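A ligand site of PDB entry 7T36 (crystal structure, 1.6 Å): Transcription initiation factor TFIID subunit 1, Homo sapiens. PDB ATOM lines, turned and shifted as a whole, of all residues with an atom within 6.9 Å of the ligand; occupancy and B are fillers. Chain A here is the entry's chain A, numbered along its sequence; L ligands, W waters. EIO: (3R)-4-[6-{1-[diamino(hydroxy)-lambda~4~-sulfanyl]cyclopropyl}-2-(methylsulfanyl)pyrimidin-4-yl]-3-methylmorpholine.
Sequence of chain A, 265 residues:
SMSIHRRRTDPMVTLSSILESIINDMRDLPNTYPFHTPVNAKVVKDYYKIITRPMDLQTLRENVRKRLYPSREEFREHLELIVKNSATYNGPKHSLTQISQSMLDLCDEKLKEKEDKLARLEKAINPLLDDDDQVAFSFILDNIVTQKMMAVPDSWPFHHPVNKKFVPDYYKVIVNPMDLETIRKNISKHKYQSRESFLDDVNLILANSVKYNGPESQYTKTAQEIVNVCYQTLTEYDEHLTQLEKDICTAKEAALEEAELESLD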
ATOM      1  N   TRP A 156     -12.945  17.932 -10.241  1.00  0.00           N
ATOM      2  CA  TRP A 156     -13.863  18.919 -10.808  1.00  0.00           C
ATOM      3  C   TRP A 156     -15.319  18.849 -10.336  1.00  0.00           C
ATOM      4  O   TRP A 156     -15.947  19.911 -10.221  1.00  0.00           O
ATOM      5  CB  TRP A 156     -13.831  18.856 -12.350  1.00  0.00           C
ATOM      6  CG  TRP A 156     -14.379  17.579 -12.935  1.00  0.00           C
ATOM      7  CD1 TRP A 156     -13.675  16.471 -13.286  1.00  0.00           C
ATOM      8  CD2 TRP A 156     -15.761  17.287 -13.208  1.00  0.00           C
ATOM      9  NE1 TRP A 156     -14.519  15.499 -13.765  1.00  0.00           N
ATOM     10  CE2 TRP A 156     -15.805  15.982 -13.741  1.00  0.00           C
ATOM     11  CE3 TRP A 156     -16.954  17.993 -13.069  1.00  0.00           C
ATOM     12  CZ2 TRP A 156     -17.000  15.372 -14.117  1.00  0.00           C
ATOM     13  CZ3 TRP A 156     -18.144  17.390 -13.442  1.00  0.00           C
ATOM     14  CH2 TRP A 156     -18.163  16.086 -13.958  1.00  0.00           C
ATOM     15  N   PRO A 157     -15.914  17.676 -10.059  1.00  0.00           N
ATOM     16  CA  PRO A 157     -17.307  17.673  -9.572  1.00  0.00           C
ATOM     17  C   PRO A 157     -17.495  18.419  -8.274  1.00  0.00           C
ATOM     18  O   PRO A 157     -18.623  18.807  -7.944  1.00  0.00           O
ATOM     19  CB  PRO A 157     -17.640  16.187  -9.412  1.00  0.00           C
ATOM     20  CG  PRO A 157     -16.638  15.471 -10.244  1.00  0.00           C
ATOM     21  CD  PRO A 157     -15.401  16.291 -10.134  1.00  0.00           C
ATOM     22  N   PHE A 158     -16.420  18.643  -7.534  1.00  0.00           N
ATOM     23  CA  PHE A 158     -16.480  19.224  -6.206  1.00  0.00           C
ATOM     24  C   PHE A 158     -15.943  20.647  -6.168  1.00  0.00           C
ATOM     25  O   PHE A 158     -15.892  21.248  -5.099  1.00  0.00           O
ATOM     26  CB  PHE A 158     -15.722  18.316  -5.231  1.00  0.00           C
ATOM     27  CG  PHE A 158     -16.164  16.887  -5.292  1.00  0.00           C
ATOM     28  CD1 PHE A 158     -17.410  16.513  -4.796  1.00  0.00           C
ATOM     29  CD2 PHE A 158     -15.356  15.907  -5.868  1.00  0.00           C
ATOM     30  CE1 PHE A 158     -17.833  15.193  -4.861  1.00  0.00           C
ATOM     31  CE2 PHE A 158     -15.779  14.587  -5.932  1.00  0.00           C
ATOM     32  CZ  PHE A 158     -17.024  14.230  -5.419  1.00  0.00           C
ATOM     33  N   HIS A 159     -15.563  21.194  -7.324  1.00  0.00           N
ATOM     34  CA  HIS A 159     -14.975  22.536  -7.365  1.00  0.00           C
ATOM     35  C   HIS A 159     -16.006  23.643  -7.219  1.00  0.00           C
ATOM     36  O   HIS A 159     -15.674  24.733  -6.744  1.00  0.00           O
ATOM     37  CB  HIS A 159     -14.216  22.740  -8.674  1.00  0.00           C
ATOM     38  CG  HIS A 159     -12.881  22.056  -8.720  1.00  0.00           C
ATOM     39  ND1 HIS A 159     -11.907  22.409  -9.630  1.00  0.00           N
ATOM     40  CD2 HIS A 159     -12.371  21.037  -7.988  1.00  0.00           C
ATOM     41  CE1 HIS A 159     -10.839  21.646  -9.440  1.00  0.00           C
ATOM     42  NE2 HIS A 159     -11.100  20.809  -8.448  1.00  0.00           N
ATOM     43  N   HIS A 160     -17.240  23.402  -7.656  1.00  0.00           N
ATOM     44  CA  HIS A 160     -18.246  24.446  -7.773  1.00  0.00           C
ATOM     45  C   HIS A 160     -19.584  23.883  -7.327  1.00  0.00           C
ATOM     46  O   HIS A 160     -19.771  22.660  -7.295  1.00  0.00           O
ATOM     47  CB  HIS A 160     -18.379  24.946  -9.223  1.00  0.00           C
ATOM     48  CG  HIS A 160     -17.115  25.532  -9.765  1.00  0.00           C
ATOM     49  ND1 HIS A 160     -16.678  26.798  -9.424  1.00  0.00           N
ATOM     50  CD2 HIS A 160     -16.196  25.022 -10.614  1.00  0.00           C
ATOM     51  CE1 HIS A 160     -15.539  27.048 -10.050  1.00  0.00           C
ATOM     52  NE2 HIS A 160     -15.219  25.984 -10.775  1.00  0.00           N
ATOM     53  N   PRO A 161     -20.545  24.746  -6.987  1.00  0.00           N
ATOM     54  CA  PRO A 161     -21.894  24.253  -6.693  1.00  0.00           C
ATOM     55  C   PRO A 161     -22.493  23.554  -7.898  1.00  0.00           C
ATOM     56  O   PRO A 161     -22.290  23.964  -9.053  1.00  0.00           O
ATOM     57  CB  PRO A 161     -22.684  25.512  -6.324  1.00  0.00           C
ATOM     58  CG  PRO A 161     -21.661  26.544  -6.021  1.00  0.00           C
ATOM     59  CD  PRO A 161     -20.431  26.201  -6.809  1.00  0.00           C
ATOM     60  N   VAL A 162     -23.245  22.491  -7.632  1.00  0.00           N
ATOM     61  CA  VAL A 162     -23.974  21.782  -8.676  1.00  0.00           C
ATOM     62  C   VAL A 162     -25.022  22.713  -9.259  1.00  0.00           C
ATOM     63  O   VAL A 162     -25.772  23.383  -8.524  1.00  0.00           O
ATOM     64  CB  VAL A 162     -24.628  20.510  -8.111  1.00  0.00           C
ATOM     65  CG1 VAL A 162     -25.598  19.912  -9.121  1.00  0.00           C
ATOM     66  CG2 VAL A 162     -23.561  19.491  -7.703  1.00  0.00           C
ATOM     67  N   ASN A 163     -25.094  22.756 -10.586  1.00  0.00           N
ATOM     68  CA  ASN A 163     -26.138  23.510 -11.280  1.00  0.00           C
ATOM     69  C   ASN A 163     -27.317  22.568 -11.502  1.00  0.00           C
ATOM     70  O   ASN A 163     -27.184  21.572 -12.217  1.00  0.00           O
ATOM     71  CB  ASN A 163     -25.610  24.076 -12.589  1.00  0.00           C
ATOM     72  CG  ASN A 163     -26.547  25.088 -13.206  1.00  0.00           C
ATOM     73  OD1 ASN A 163     -27.765  24.926 -13.151  1.00  0.00           O
ATOM     74  ND2 ASN A 163     -25.998  26.137 -13.814  1.00  0.00           N
ATOM     75  N   LYS A 164     -28.456  22.887 -10.885  1.00  0.00           N
ATOM     76  CA  LYS A 164     -29.653  22.054 -11.001  1.00  0.00           C
ATOM     77  C   LYS A 164     -30.052  21.812 -12.452  1.00  0.00           C
ATOM     78  O   LYS A 164     -30.685  20.801 -12.766  1.00  0.00           O
ATOM     79  CB  LYS A 164     -30.812  22.727 -10.251  1.00  0.00           C
ATOM     80  CG  LYS A 164     -32.030  21.826 -10.038  1.00  0.00           C
ATOM     81  CD  LYS A 164     -33.209  22.611  -9.483  1.00  0.00           C
ATOM     82  CE  LYS A 164     -32.922  23.205  -8.136  1.00  0.00           C
ATOM     83  NZ  LYS A 164     -34.186  23.657  -7.514  1.00  0.00           N
ATOM     84  N   LYS A 165     -29.703  22.732 -13.364  1.00  0.00           N
ATOM     85  CA  LYS A 165     -30.048  22.528 -14.759  1.00  0.00           C
ATOM     86  C   LYS A 165     -29.376  21.281 -15.323  1.00  0.00           C
ATOM     87  O   LYS A 165     -29.954  20.571 -16.161  1.00  0.00           O
ATOM     88  CB  LYS A 165     -29.664  23.744 -15.588  1.00  0.00           C
ATOM     89  CG  LYS A 165     -30.041  23.632 -17.035  1.00  0.00           C
ATOM     90  CD  LYS A 165     -29.807  24.930 -17.775  1.00  0.00           C
ATOM     91  CE  LYS A 165     -30.320  24.837 -19.193  1.00  0.00           C
ATOM     92  NZ  LYS A 165     -30.010  26.069 -19.969  1.00  0.00           N
ATOM     93  N   PHE A 166     -28.163  20.975 -14.865  1.00  0.00           N
ATOM     94  CA  PHE A 166     -27.398  19.853 -15.389  1.00  0.00           C
ATOM     95  C   PHE A 166     -27.535  18.583 -14.553  1.00  0.00           C
ATOM     96  O   PHE A 166     -27.297  17.490 -15.070  1.00  0.00           O
ATOM     97  CB  PHE A 166     -25.918  20.234 -15.495  1.00  0.00           C
ATOM     98  CG  PHE A 166     -25.671  21.483 -16.291  1.00  0.00           C
ATOM     99  CD1 PHE A 166     -26.414  21.729 -17.447  1.00  0.00           C
ATOM    100  CD2 PHE A 166     -24.708  22.400 -15.910  1.00  0.00           C
ATOM    101  CE1 PHE A 166     -26.199  22.884 -18.195  1.00  0.00           C
ATOM    102  CE2 PHE A 166     -24.493  23.555 -16.658  1.00  0.00           C
ATOM    103  CZ  PHE A 166     -25.230  23.792 -17.805  1.00  0.00           C
ATOM    104  N   VAL A 167     -27.909  18.711 -13.273  1.00  0.00           N
ATOM    105  CA  VAL A 167     -28.165  17.566 -12.402  1.00  0.00           C
ATOM    106  C   VAL A 167     -29.517  17.815 -11.727  1.00  0.00           C
ATOM    107  O   VAL A 167     -29.558  18.274 -10.586  1.00  0.00           O
ATOM    108  CB  VAL A 167     -27.038  17.385 -11.363  1.00  0.00           C
ATOM    109  CG1 VAL A 167     -27.198  16.053 -10.639  1.00  0.00           C
ATOM    110  CG2 VAL A 167     -25.658  17.475 -12.029  1.00  0.00           C
ATOM    111  N   TYR A 170     -30.414  16.794  -7.949  1.00  0.00           N
ATOM    112  CA  TYR A 170     -29.328  16.845  -6.962  1.00  0.00           C
ATOM    113  C   TYR A 170     -29.807  17.399  -5.621  1.00  0.00           C
ATOM    114  O   TYR A 170     -29.497  16.842  -4.568  1.00  0.00           O
ATOM    115  CB  TYR A 170     -28.161  17.683  -7.486  1.00  0.00           C
ATOM    116  CG  TYR A 170     -26.969  17.626  -6.575  1.00  0.00           C
ATOM    117  CD1 TYR A 170     -26.124  16.517  -6.570  1.00  0.00           C
ATOM    118  CD2 TYR A 170     -26.704  18.652  -5.684  1.00  0.00           C
ATOM    119  CE1 TYR A 170     -25.041  16.449  -5.719  1.00  0.00           C
ATOM    120  CE2 TYR A 170     -25.617  18.589  -4.820  1.00  0.00           C
ATOM    121  CZ  TYR A 170     -24.787  17.493  -4.846  1.00  0.00           C
ATOM    122  OH  TYR A 170     -23.720  17.437  -3.995  1.00  0.00           O
ATOM    123  N   ASP A 179     -19.176  22.853  -1.584  1.00  0.00           N
ATOM    124  CA  ASP A 179     -18.192  22.669  -2.645  1.00  0.00           C
ATOM    125  C   ASP A 179     -16.976  23.526  -2.334  1.00  0.00           C
ATOM    126  O   ASP A 179     -17.008  24.387  -1.447  1.00  0.00           O
ATOM    127  CB  ASP A 179     -18.785  23.070  -3.985  1.00  0.00           C
ATOM    128  CG  ASP A 179     -19.132  24.528  -4.009  1.00  0.00           C
ATOM    129  OD1 ASP A 179     -20.221  24.866  -3.503  1.00  0.00           O
ATOM    130  OD2 ASP A 179     -18.290  25.331  -4.459  1.00  0.00           O
ATOM    131  N   ILE A 205     -18.629  17.936   1.912  1.00  0.00           N
ATOM    132  CA  ILE A 205     -18.441  17.544   0.525  1.00  0.00           C
ATOM    133  C   ILE A 205     -18.431  16.019   0.407  1.00  0.00           C
ATOM    134  O   ILE A 205     -19.096  15.444  -0.461  1.00  0.00           O
ATOM    135  CB  ILE A 205     -17.143  18.157  -0.043  1.00  0.00           C
ATOM    136  CG1 ILE A 205     -17.211  19.688   0.043  1.00  0.00           C
ATOM    137  CG2 ILE A 205     -16.962  17.740  -1.504  1.00  0.00           C
ATOM    138  CD1 ILE A 205     -15.948  20.386  -0.398  1.00  0.00           C
ATOM    139  N   ASN A 208     -21.877  14.409   1.297  1.00  0.00           N
ATOM    140  CA  ASN A 208     -22.846  14.568   0.223  1.00  0.00           C
ATOM    141  C   ASN A 208     -22.559  13.619  -0.925  1.00  0.00           C
ATOM    142  O   ASN A 208     -23.495  13.144  -1.586  1.00  0.00           O
ATOM    143  CB  ASN A 208     -22.862  16.011  -0.269  1.00  0.00           C
ATOM    144  CG  ASN A 208     -23.465  16.958   0.741  1.00  0.00           C
ATOM    145  OD1 ASN A 208     -24.253  16.555   1.602  1.00  0.00           O
ATOM    146  ND2 ASN A 208     -23.101  18.234   0.659  1.00  0.00           N
ATOM    147  N   SER A 209     -21.278  13.333  -1.177  1.00  0.00           N
ATOM    148  CA  SER A 209     -20.954  12.381  -2.242  1.00  0.00           C
ATOM    149  C   SER A 209     -21.391  10.985  -1.861  1.00  0.00           C
ATOM    150  O   SER A 209     -21.905  10.227  -2.700  1.00  0.00           O
ATOM    151  CB  SER A 209     -19.453  12.409  -2.534  1.00  0.00           C
ATOM    152  OG  SER A 209     -19.145  11.570  -3.641  1.00  0.00           O
ATOM    153  N   TYR A 212     -25.243  11.064  -2.397  1.00  0.00           N
ATOM    154  CA  TYR A 212     -25.763  11.179  -3.760  1.00  0.00           C
ATOM    155  C   TYR A 212     -25.192  10.103  -4.679  1.00  0.00           C
ATOM    156  O   TYR A 212     -25.923   9.522  -5.489  1.00  0.00           O
ATOM    157  CB  TYR A 212     -25.490  12.559  -4.345  1.00  0.00           C
ATOM    158  CG  TYR A 212     -26.200  12.734  -5.678  1.00  0.00           C
ATOM    159  CD1 TYR A 212     -27.552  13.030  -5.720  1.00  0.00           C
ATOM    160  CD2 TYR A 212     -25.527  12.555  -6.874  1.00  0.00           C
ATOM    161  CE1 TYR A 212     -28.214  13.168  -6.915  1.00  0.00           C
ATOM    162  CE2 TYR A 212     -26.190  12.691  -8.091  1.00  0.00           C
ATOM    163  CZ  TYR A 212     -27.531  13.000  -8.094  1.00  0.00           C
ATOM    164  OH  TYR A 212     -28.191  13.141  -9.298  1.00  0.00           O
ATOM    165  N   ASN A 213     -23.890   9.823  -4.568  1.00  0.00           N
ATOM    166  CA  ASN A 213     -23.228   8.904  -5.480  1.00  0.00           C
ATOM    167  C   ASN A 213     -23.079   7.504  -4.923  1.00  0.00           C
ATOM    168  O   ASN A 213     -22.931   6.562  -5.713  1.00  0.00           O
ATOM    169  CB  ASN A 213     -21.846   9.442  -5.860  1.00  0.00           C
ATOM    170  CG  ASN A 213     -21.925  10.820  -6.451  1.00  0.00           C
ATOM    171  OD1 ASN A 213     -22.656  11.044  -7.418  1.00  0.00           O
ATOM    172  ND2 ASN A 213     -21.204  11.777  -5.866  1.00  0.00           N
ATOM    173  N   SER A 217     -18.716   4.659  -5.096  1.00  0.00           N
ATOM    174  CA  SER A 217     -18.619   5.347  -6.378  1.00  0.00           C
ATOM    175  C   SER A 217     -17.232   5.939  -6.577  1.00  0.00           C
ATOM    176  O   SER A 217     -16.546   6.307  -5.622  1.00  0.00           O
ATOM    177  CB  SER A 217     -19.668   6.451  -6.442  1.00  0.00           C
ATOM    178  OG  SER A 217     -19.364   7.430  -7.431  1.00  0.00           O
ATOM    179  N   TYR A 219     -16.774   8.836  -7.810  1.00  0.00           N
ATOM    180  CA  TYR A 219     -16.900  10.197  -7.298  1.00  0.00           C
ATOM    181  C   TYR A 219     -16.547  10.259  -5.819  1.00  0.00           C
ATOM    182  O   TYR A 219     -15.851  11.185  -5.378  1.00  0.00           O
ATOM    183  CB  TYR A 219     -18.335  10.718  -7.501  1.00  0.00           C
ATOM    184  CG  TYR A 219     -18.644  11.099  -8.933  1.00  0.00           C
ATOM    185  CD1 TYR A 219     -17.747  11.847  -9.678  1.00  0.00           C
ATOM    186  CD2 TYR A 219     -19.836  10.716  -9.526  1.00  0.00           C
ATOM    187  CE1 TYR A 219     -18.025  12.201 -10.994  1.00  0.00           C
ATOM    188  CE2 TYR A 219     -20.128  11.068 -10.845  1.00  0.00           C
ATOM    189  CZ  TYR A 219     -19.216  11.818 -11.565  1.00  0.00           C
ATOM    190  OH  TYR A 219     -19.482  12.170 -12.868  1.00  0.00           O
HETATM  191  C13 EIO L   1     -23.465  14.864  -9.373  1.00  0.00           C
HETATM  192  C15 EIO L   1     -21.731  17.451 -12.717  1.00  0.00           C
HETATM  193  C17 EIO L   1     -22.479  14.949 -14.082  1.00  0.00           C
HETATM  194  C20 EIO L   1     -19.246  21.200 -11.613  1.00  0.00           C
HETATM  195  C03 EIO L   1     -20.661  20.701 -11.315  1.00  0.00           C
HETATM  196  C04 EIO L   1     -21.043  19.221 -11.444  1.00  0.00           C
HETATM  197  C05 EIO L   1     -20.996  18.393 -10.314  1.00  0.00           C
HETATM  198  C06 EIO L   1     -21.357  17.059 -10.498  1.00  0.00           C
HETATM  199  C08 EIO L   1     -21.939  14.773  -9.547  1.00  0.00           C
HETATM  200  C09 EIO L   1     -21.356  13.779  -8.542  1.00  0.00           C
HETATM  201  C11 EIO L   1     -20.774  15.471  -7.060  1.00  0.00           C
HETATM  202  C12 EIO L   1     -21.349  16.556  -7.990  1.00  0.00           C
HETATM  203  C19 EIO L   1     -19.920  21.577 -10.299  1.00  0.00           C
HETATM  204  N01 EIO L   1     -22.006  23.245 -12.064  1.00  0.00           N
HETATM  205  N07 EIO L   1     -21.338  16.111  -9.382  1.00  0.00           N
HETATM  206  N14 EIO L   1     -21.715  16.618 -11.693  1.00  0.00           N
HETATM  207  N18 EIO L   1     -21.408  18.736 -12.622  1.00  0.00           N
HETATM  208  N21 EIO L   1     -22.247  21.445 -13.708  1.00  0.00           N
HETATM  209  O10 EIO L   1     -21.458  14.272  -7.242  1.00  0.00           O
HETATM  210  O22 EIO L   1     -23.281  21.254 -12.307  1.00  0.00           O
HETATM  211  S02 EIO L   1     -21.892  21.710 -12.237  1.00  0.00           S
HETATM  212  S16 EIO L   1     -22.238  16.749 -14.301  1.00  0.00           S
HETATM  213  O   HOH W   1     -15.972  22.067 -11.913  1.00  0.00           O
HETATM  214  O   HOH W   2     -22.948  26.085 -10.450  1.00  0.00           O
HETATM  215  O   HOH W   3     -21.869  24.527 -14.543  1.00  0.00           O
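Water W2 lies within hydrogen-bond range of the backbone carbonyl oxygen of Pro 161 (2.6 Å) and a nitrogen (N01) of the ligand (3.4 Å).
An oxygen (O22) of the ligand sits at hydrogen-bond distance from the backbone NH (N) of Asn 163, 2.9 Å away.
The side-chain amide nitrogen (ND2) of Asn 213 lies within hydrogen-bond range of an oxygen (O10) of the ligand.
A nitrogen (N01) of the ligand lies within hydrogen-bond range of the backbone carbonyl oxygen (O) of Pro 161 (3.1 Å).
The backbone NH (N) of Tyr 219 sits at hydrogen-bond distance from the side-chain hydroxyl (OG) of Ser 217 (3.0 Å).
OG of Ser 209 is in hydrogen-bond range of ND2 of Asn 213 (3.0 Å).
The backbone NH (N) of Lys 165 is in hydrogen-bond range of the side-chain amide oxygen (OD1) of Asn 163.
CZ3 of Trp 156 touches N18 of the ligand (3.6 Å).
Pro 157 touches the ligand.
CE1 of Phe 158 touches C11 of the ligand (3.7 Å).
His 160 touches the ligand.
Val 162 touches the ligand (CG2 to C12, 3.7 Å).
Phe 166 touches the ligand (CD2 to N21, 3.4 Å).
Val 167 touches the ligand (CG2 to C15, 3.99 Å).
CE2 of Tyr 212 touches C13 of the ligand (3.7 Å).
CD2 of Tyr 219 touches C09 of the ligand, at 3.6 Å.
Hydrophobic or aromatic side chains within 4 Å of the ligand: Trp 156, Pro 157, Phe 158, His 160, Val 162, Phe 166, Val 167, Tyr 212 and Tyr 219.
Of the 21 residues printed, 12 come within 4 Å of the ligand.
The nearest printed residue that does not touch the ligand is Tyr 170 (4.2 Å).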
